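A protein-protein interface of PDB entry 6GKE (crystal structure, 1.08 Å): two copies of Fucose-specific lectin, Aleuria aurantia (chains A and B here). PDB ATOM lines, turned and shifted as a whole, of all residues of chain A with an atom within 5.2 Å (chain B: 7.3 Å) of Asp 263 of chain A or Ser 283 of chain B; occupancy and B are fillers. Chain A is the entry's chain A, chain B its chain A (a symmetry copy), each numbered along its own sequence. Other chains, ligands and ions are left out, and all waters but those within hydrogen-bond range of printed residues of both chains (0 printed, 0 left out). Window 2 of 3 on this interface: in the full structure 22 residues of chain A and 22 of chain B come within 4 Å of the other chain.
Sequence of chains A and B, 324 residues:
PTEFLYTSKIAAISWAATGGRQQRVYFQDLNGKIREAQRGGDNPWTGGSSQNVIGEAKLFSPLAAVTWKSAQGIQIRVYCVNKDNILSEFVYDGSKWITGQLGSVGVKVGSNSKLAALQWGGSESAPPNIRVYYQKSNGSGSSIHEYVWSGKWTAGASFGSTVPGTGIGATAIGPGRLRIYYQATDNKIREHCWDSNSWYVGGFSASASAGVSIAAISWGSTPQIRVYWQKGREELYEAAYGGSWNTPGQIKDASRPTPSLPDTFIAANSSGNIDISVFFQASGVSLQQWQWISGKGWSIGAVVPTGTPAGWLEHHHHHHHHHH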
ATOM      1  N   TYR A   6       9.054  -3.051  21.789  1.00  0.00           N
ATOM      2  CA  TYR A   6       8.847  -2.396  23.077  1.00  0.00           C
ATOM      3  C   TYR A   6       8.571  -3.467  24.132  1.00  0.00           C
ATOM      4  O   TYR A   6       7.689  -4.300  23.940  1.00  0.00           O
ATOM      5  CB  TYR A   6       7.699  -1.389  23.007  1.00  0.00           C
ATOM      6  CG  TYR A   6       7.295  -0.808  24.336  1.00  0.00           C
ATOM      7  CD1 TYR A   6       8.211  -0.155  25.144  1.00  0.00           C
ATOM      8  CD2 TYR A   6       5.992  -0.918  24.785  1.00  0.00           C
ATOM      9  CE1 TYR A   6       7.839   0.387  26.363  1.00  0.00           C
ATOM     10  CE2 TYR A   6       5.600  -0.370  25.994  1.00  0.00           C
ATOM     11  CZ  TYR A   6       6.529   0.274  26.789  1.00  0.00           C
ATOM     12  OH  TYR A   6       6.120   0.810  27.978  1.00  0.00           O
ATOM     13  N   THR A   7       9.328  -3.402  25.229  1.00  0.00           N
ATOM     14  CA  THR A   7       9.344  -4.377  26.348  1.00  0.00           C
ATOM     15  C   THR A   7      10.017  -5.692  25.940  1.00  0.00           C
ATOM     16  O   THR A   7       9.921  -6.686  26.659  1.00  0.00           O
ATOM     17  CB  THR A   7       7.988  -4.594  27.050  1.00  0.00           C
ATOM     18  OG1 THR A   7       7.085  -5.388  26.279  1.00  0.00           O
ATOM     19  CG2 THR A   7       7.333  -3.288  27.433  1.00  0.00           C
ATOM     20  N   GLY A 232      11.038   0.220  35.070  1.00  0.00           N
ATOM     21  CA  GLY A 232      10.948   1.125  33.944  1.00  0.00           C
ATOM     22  C   GLY A 232      10.416   2.481  34.381  1.00  0.00           C
ATOM     23  O   GLY A 232       9.456   2.565  35.148  1.00  0.00           O
ATOM     24  N   LEU A 261      11.676   3.746  29.467  1.00  0.00           N
ATOM     25  CA  LEU A 261      10.227   3.693  29.351  1.00  0.00           C
ATOM     26  C   LEU A 261       9.632   2.777  30.415  1.00  0.00           C
ATOM     27  O   LEU A 261      10.293   1.881  30.944  1.00  0.00           O
ATOM     28  CB  LEU A 261       9.821   3.200  27.961  1.00  0.00           C
ATOM     29  CG  LEU A 261      10.055   4.172  26.808  1.00  0.00           C
ATOM     30  CD1 LEU A 261       9.908   3.439  25.487  1.00  0.00           C
ATOM     31  CD2 LEU A 261       9.101   5.359  26.874  1.00  0.00           C
ATOM     32  N   PRO A 262       8.327   2.942  30.726  1.00  0.00           N
ATOM     33  CA  PRO A 262       7.656   2.018  31.638  1.00  0.00           C
ATOM     34  C   PRO A 262       7.780   0.559  31.180  1.00  0.00           C
ATOM     35  O   PRO A 262       7.761   0.270  29.980  1.00  0.00           O
ATOM     36  CB  PRO A 262       6.197   2.493  31.606  1.00  0.00           C
ATOM     37  CG  PRO A 262       6.309   3.959  31.269  1.00  0.00           C
ATOM     38  CD  PRO A 262       7.434   4.019  30.260  1.00  0.00           C
ATOM     39  N   ASP A 263       7.898  -0.342  32.161  1.00  0.00           N
ATOM     40  CA  ASP A 263       7.729  -1.798  31.975  1.00  0.00           C
ATOM     41  C   ASP A 263       8.847  -2.409  31.119  1.00  0.00           C
ATOM     42  O   ASP A 263       8.701  -3.517  30.610  1.00  0.00           O
ATOM     43  CB  ASP A 263       6.351  -2.117  31.391  1.00  0.00           C
ATOM     44  CG  ASP A 263       5.244  -1.592  32.279  1.00  0.00           C
ATOM     45  OD1 ASP A 263       5.265  -1.910  33.484  1.00  0.00           O
ATOM     46  OD2 ASP A 263       4.380  -0.851  31.774  1.00  0.00           O
ATOM     47  N   THR A 264       9.999  -1.735  31.054  1.00  0.00           N
ATOM     48  CA  THR A 264      11.138  -2.168  30.258  1.00  0.00           C
ATOM     49  C   THR A 264      12.168  -2.890  31.134  1.00  0.00           C
ATOM     50  O   THR A 264      12.081  -2.915  32.358  1.00  0.00           O
ATOM     51  CB  THR A 264      11.771  -0.976  29.533  1.00  0.00           C
ATOM     52  OG1 THR A 264      12.185  -0.023  30.511  1.00  0.00           O
ATOM     53  CG2 THR A 264      10.828  -0.353  28.529  1.00  0.00           C
ATOM     54  N   PHE A 265      13.173  -3.459  30.467  1.00  0.00           N
ATOM     55  CA  PHE A 265      14.164  -4.333  31.097  1.00  0.00           C
ATOM     56  C   PHE A 265      15.572  -3.748  30.980  1.00  0.00           C
ATOM     57  O   PHE A 265      15.826  -2.861  30.166  1.00  0.00           O
ATOM     58  CB  PHE A 265      14.084  -5.720  30.453  1.00  0.00           C
ATOM     59  CG  PHE A 265      12.731  -6.347  30.659  1.00  0.00           C
ATOM     60  CD1 PHE A 265      12.397  -6.911  31.881  1.00  0.00           C
ATOM     61  CD2 PHE A 265      11.755  -6.286  29.678  1.00  0.00           C
ATOM     62  CE1 PHE A 265      11.130  -7.427  32.108  1.00  0.00           C
ATOM     63  CE2 PHE A 265      10.489  -6.804  29.908  1.00  0.00           C
ATOM     64  CZ  PHE A 265      10.177  -7.367  31.123  1.00  0.00           C
ATOM     65  N   THR B   2       0.381  -8.053  24.372  1.00  0.00           N
ATOM     66  CA  THR B   2      -0.598  -8.088  23.299  1.00  0.00           C
ATOM     67  C   THR B   2       0.120  -7.914  21.961  1.00  0.00           C
ATOM     68  O   THR B   2       1.341  -7.759  21.914  1.00  0.00           O
ATOM     69  CB  THR B   2      -1.676  -7.007  23.463  1.00  0.00           C
ATOM     70  OG1 THR B   2      -1.110  -5.770  23.026  1.00  0.00           O
ATOM     71  CG2 THR B   2      -2.201  -6.897  24.879  1.00  0.00           C
ATOM     72  N   ARG B 256      -6.338   7.075  38.530  1.00  0.00           N
ATOM     73  CA  ARG B 256      -5.561   6.584  37.391  1.00  0.00           C
ATOM     74  C   ARG B 256      -4.940   7.770  36.664  1.00  0.00           C
ATOM     75  O   ARG B 256      -5.320   8.090  35.535  1.00  0.00           O
ATOM     76  CB  ARG B 256      -6.445   5.752  36.460  1.00  0.00           C
ATOM     77  CG  ARG B 256      -6.902   4.442  37.084  1.00  0.00           C
ATOM     78  CD  ARG B 256      -7.683   3.572  36.125  1.00  0.00           C
ATOM     79  NE  ARG B 256      -6.899   3.174  34.965  1.00  0.00           N
ATOM     80  CZ  ARG B 256      -7.375   2.448  33.966  1.00  0.00           C
ATOM     81  NH1 ARG B 256      -8.608   1.977  34.033  1.00  0.00           N
ATOM     82  NH2 ARG B 256      -6.625   2.205  32.904  1.00  0.00           N
ATOM     83  N   PRO B 259      -2.981   8.044  32.291  1.00  0.00           N
ATOM     84  CA  PRO B 259      -2.964   6.601  32.067  1.00  0.00           C
ATOM     85  C   PRO B 259      -2.344   6.112  30.749  1.00  0.00           C
ATOM     86  O   PRO B 259      -2.162   4.910  30.608  1.00  0.00           O
ATOM     87  CB  PRO B 259      -4.455   6.223  32.134  1.00  0.00           C
ATOM     88  CG  PRO B 259      -5.174   7.473  31.691  1.00  0.00           C
ATOM     89  CD  PRO B 259      -4.343   8.601  32.263  1.00  0.00           C
ATOM     90  N   SER B 260      -2.043   7.016  29.810  1.00  0.00           N
ATOM     91  CA  SER B 260      -1.430   6.617  28.546  1.00  0.00           C
ATOM     92  C   SER B 260       0.090   6.492  28.690  1.00  0.00           C
ATOM     93  O   SER B 260       0.701   7.087  29.565  1.00  0.00           O
ATOM     94  CB  SER B 260      -1.764   7.578  27.440  1.00  0.00           C
ATOM     95  OG  SER B 260      -1.210   8.868  27.676  1.00  0.00           O
ATOM     96  N   LEU B 261       0.692   5.724  27.780  1.00  0.00           N
ATOM     97  CA  LEU B 261       2.142   5.618  27.710  1.00  0.00           C
ATOM     98  C   LEU B 261       2.737   6.814  26.975  1.00  0.00           C
ATOM     99  O   LEU B 261       2.076   7.480  26.175  1.00  0.00           O
ATOM    100  CB  LEU B 261       2.549   4.325  27.001  1.00  0.00           C
ATOM    101  CG  LEU B 261       2.315   3.031  27.777  1.00  0.00           C
ATOM    102  CD1 LEU B 261       2.462   1.844  26.843  1.00  0.00           C
ATOM    103  CD2 LEU B 261       3.268   2.907  28.960  1.00  0.00           C
ATOM    104  N   PHE B 280      -7.032   5.535  23.673  1.00  0.00           N
ATOM    105  CA  PHE B 280      -5.641   5.793  23.987  1.00  0.00           C
ATOM    106  C   PHE B 280      -4.919   4.459  24.201  1.00  0.00           C
ATOM    107  O   PHE B 280      -5.540   3.397  24.292  1.00  0.00           O
ATOM    108  CB  PHE B 280      -5.518   6.733  25.194  1.00  0.00           C
ATOM    109  CG  PHE B 280      -6.014   6.213  26.521  1.00  0.00           C
ATOM    110  CD1 PHE B 280      -7.340   6.375  26.903  1.00  0.00           C
ATOM    111  CD2 PHE B 280      -5.143   5.613  27.417  1.00  0.00           C
ATOM    112  CE1 PHE B 280      -7.783   5.933  28.141  1.00  0.00           C
ATOM    113  CE2 PHE B 280      -5.586   5.170  28.653  1.00  0.00           C
ATOM    114  CZ  PHE B 280      -6.903   5.331  29.013  1.00  0.00           C
ATOM    115  N   GLN B 281      -3.587   4.537  24.262  1.00  0.00           N
ATOM    116  CA  GLN B 281      -2.744   3.355  24.402  1.00  0.00           C
ATOM    117  C   GLN B 281      -2.015   3.413  25.744  1.00  0.00           C
ATOM    118  O   GLN B 281      -1.360   4.405  26.064  1.00  0.00           O
ATOM    119  CB  GLN B 281      -1.762   3.254  23.235  1.00  0.00           C
ATOM    120  CG  GLN B 281      -0.870   2.020  23.301  1.00  0.00           C
ATOM    121  CD  GLN B 281       0.019   1.907  22.086  1.00  0.00           C
ATOM    122  OE1 GLN B 281       0.835   2.784  21.813  1.00  0.00           O
ATOM    123  NE2 GLN B 281      -0.144   0.833  21.324  1.00  0.00           N
ATOM    124  N   ALA B 282      -2.109   2.309  26.494  1.00  0.00           N
ATOM    125  CA  ALA B 282      -1.599   2.218  27.852  1.00  0.00           C
ATOM    126  C   ALA B 282      -0.733   0.965  28.004  1.00  0.00           C
ATOM    127  O   ALA B 282      -0.608   0.155  27.090  1.00  0.00           O
ATOM    128  CB  ALA B 282      -2.751   2.187  28.824  1.00  0.00           C
ATOM    129  N   SER B 283      -0.145   0.809  29.192  1.00  0.00           N
ATOM    130  CA  SER B 283       0.617  -0.388  29.513  1.00  0.00           C
ATOM    131  C   SER B 283      -0.243  -1.627  29.248  1.00  0.00           C
ATOM    132  O   SER B 283      -1.457  -1.616  29.434  1.00  0.00           O
ATOM    133  CB  SER B 283       1.106  -0.364  30.933  1.00  0.00           C
ATOM    134  OG  SER B 283       0.015  -0.422  31.836  1.00  0.00           O
ATOM    135  N   GLY B 284       0.409  -2.700  28.794  1.00  0.00           N
ATOM    136  CA  GLY B 284      -0.313  -3.919  28.455  1.00  0.00           C
ATOM    137  C   GLY B 284       0.384  -4.741  27.376  1.00  0.00           C
ATOM    138  O   GLY B 284       0.724  -5.894  27.623  1.00  0.00           O
ATOM    139  N   VAL B 285       0.612  -4.194  26.175  1.00  0.00           N
ATOM    140  CA  VAL B 285       0.199  -2.884  25.687  1.00  0.00           C
ATOM    141  C   VAL B 285      -1.295  -2.924  25.347  1.00  0.00           C
ATOM    142  O   VAL B 285      -1.725  -3.761  24.557  1.00  0.00           O
ATOM    143  CB  VAL B 285       1.046  -2.505  24.451  1.00  0.00           C
ATOM    144  CG1 VAL B 285       0.519  -1.270  23.739  1.00  0.00           C
ATOM    145  CG2 VAL B 285       2.514  -2.326  24.805  1.00  0.00           C
ATOM    146  N   SER B 286      -2.072  -2.004  25.924  1.00  0.00           N
ATOM    147  CA  SER B 286      -3.524  -2.099  25.864  1.00  0.00           C
ATOM    148  C   SER B 286      -4.137  -0.913  25.116  1.00  0.00           C
ATOM    149  O   SER B 286      -3.595   0.196  25.097  1.00  0.00           O
ATOM    150  CB  SER B 286      -4.118  -2.234  27.244  1.00  0.00           C
ATOM    151  OG  SER B 286      -3.801  -1.117  28.059  1.00  0.00           O
ATOM    152  N   LEU B 287      -5.292  -1.195  24.504  1.00  0.00           N
ATOM    153  CA  LEU B 287      -6.144  -0.201  23.873  1.00  0.00           C
ATOM    154  C   LEU B 287      -7.296   0.092  24.833  1.00  0.00           C
ATOM    155  O   LEU B 287      -8.110  -0.783  25.133  1.00  0.00           O
ATOM    156  CB  LEU B 287      -6.630  -0.754  22.531  1.00  0.00           C
ATOM    157  CG  LEU B 287      -7.558   0.139  21.710  1.00  0.00           C
ATOM    158  CD1 LEU B 287      -6.985   1.531  21.503  1.00  0.00           C
ATOM    159  CD2 LEU B 287      -7.844  -0.516  20.369  1.00  0.00           C
ATOM    160  N   GLN B 288      -7.304   1.324  25.343  1.00  0.00           N
ATOM    161  CA  GLN B 288      -8.247   1.778  26.337  1.00  0.00           C
ATOM    162  C   GLN B 288      -9.097   2.894  25.738  1.00  0.00           C
ATOM    163  O   GLN B 288      -8.796   3.408  24.660  1.00  0.00           O
ATOM    164  CB  GLN B 288      -7.517   2.355  27.549  1.00  0.00           C
ATOM    165  CG  GLN B 288      -6.425   1.475  28.124  1.00  0.00           C
ATOM    166  CD  GLN B 288      -6.799   0.759  29.396  1.00  0.00           C
ATOM    167  OE1 GLN B 288      -7.794   1.068  30.055  1.00  0.00           O
ATOM    168  NE2 GLN B 288      -5.956  -0.190  29.764  1.00  0.00           N
ATOM    169  N   VAL B 303     -11.687  -2.407  28.294  1.00  0.00           N
ATOM    170  CA  VAL B 303     -10.470  -2.542  27.501  1.00  0.00           C
ATOM    171  C   VAL B 303     -10.827  -3.227  26.179  1.00  0.00           C
ATOM    172  O   VAL B 303     -11.604  -4.183  26.147  1.00  0.00           O
ATOM    173  CB  VAL B 303      -9.379  -3.318  28.263  1.00  0.00           C
ATOM    174  CG1 VAL B 303      -8.138  -3.543  27.413  1.00  0.00           C
ATOM    175  CG2 VAL B 303      -9.009  -2.627  29.567  1.00  0.00           C
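The backbone carbonyl oxygen (O) of Pro 262 of chain A is in hydrogen-bond range of the side-chain hydroxyl (OH) of Tyr 6 of chain A, 2.6 Å away. The side-chain hydroxyl (OG1) of Thr 2 of chain B is in hydrogen-bond range of the backbone carbonyl oxygen (O) of Val 285 of chain B (2.6 Å). The backbone NH of Leu 261 of chain B lies within hydrogen-bond range of the backbone carbonyl oxygen of Gln 281 of chain B (3.0 Å). O of Ser 283 of chain B lies within hydrogen-bond range of OG of Ser 286 of chain B.
Leu 261 of chain B touches Tyr 6 of chain A (CD2 to OH, 3.7 Å). Val 285 of chain B touches Tyr 6 of chain A (CG2 to CD2, 3.8 Å). CG of Pro 262 of chain A touches CD2 of Leu 261 of chain B (3.96 Å). Asp 263 of chain A touches Ser 283 of chain B (OD2 to CB, 3.4 Å).
Of the printed residues of chain B, Tyr 6 of chain A touches Leu 261 (3.7 Å) and Val 285 (3.8 Å). Of the printed residues of chain B, Asp 263 of chain A touches Ser 283 (3.4 Å). Ser 260 of chain B touches none of the printed residues of chain A. Of the printed residues of chain A, Leu 261 of chain B touches Tyr 6 and Pro 262. Of the printed residues of chain A, Ser 283 of chain B touches Asp 263 (3.4 Å). Gln 288 of chain B touches none of the printed residues of chain A. The nearest printed residue of chain A that does not touch Ser 283 of chain B is Tyr 6 of chain A (5.8 Å).
Printed residues of chain B that touch a printed residue of chain A: Leu 261, Ser 283 and Val 285. Hydrophobic or aromatic side chains of chain B within 4 Å of the printed part of chain A: Leu 261 and Val 285. Among the printed residues, no Asp or Glu carboxylate lies within 4 Å of a Lys or Arg side-chain nitrogen of the other chain.
Position printed for both chains: 261.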
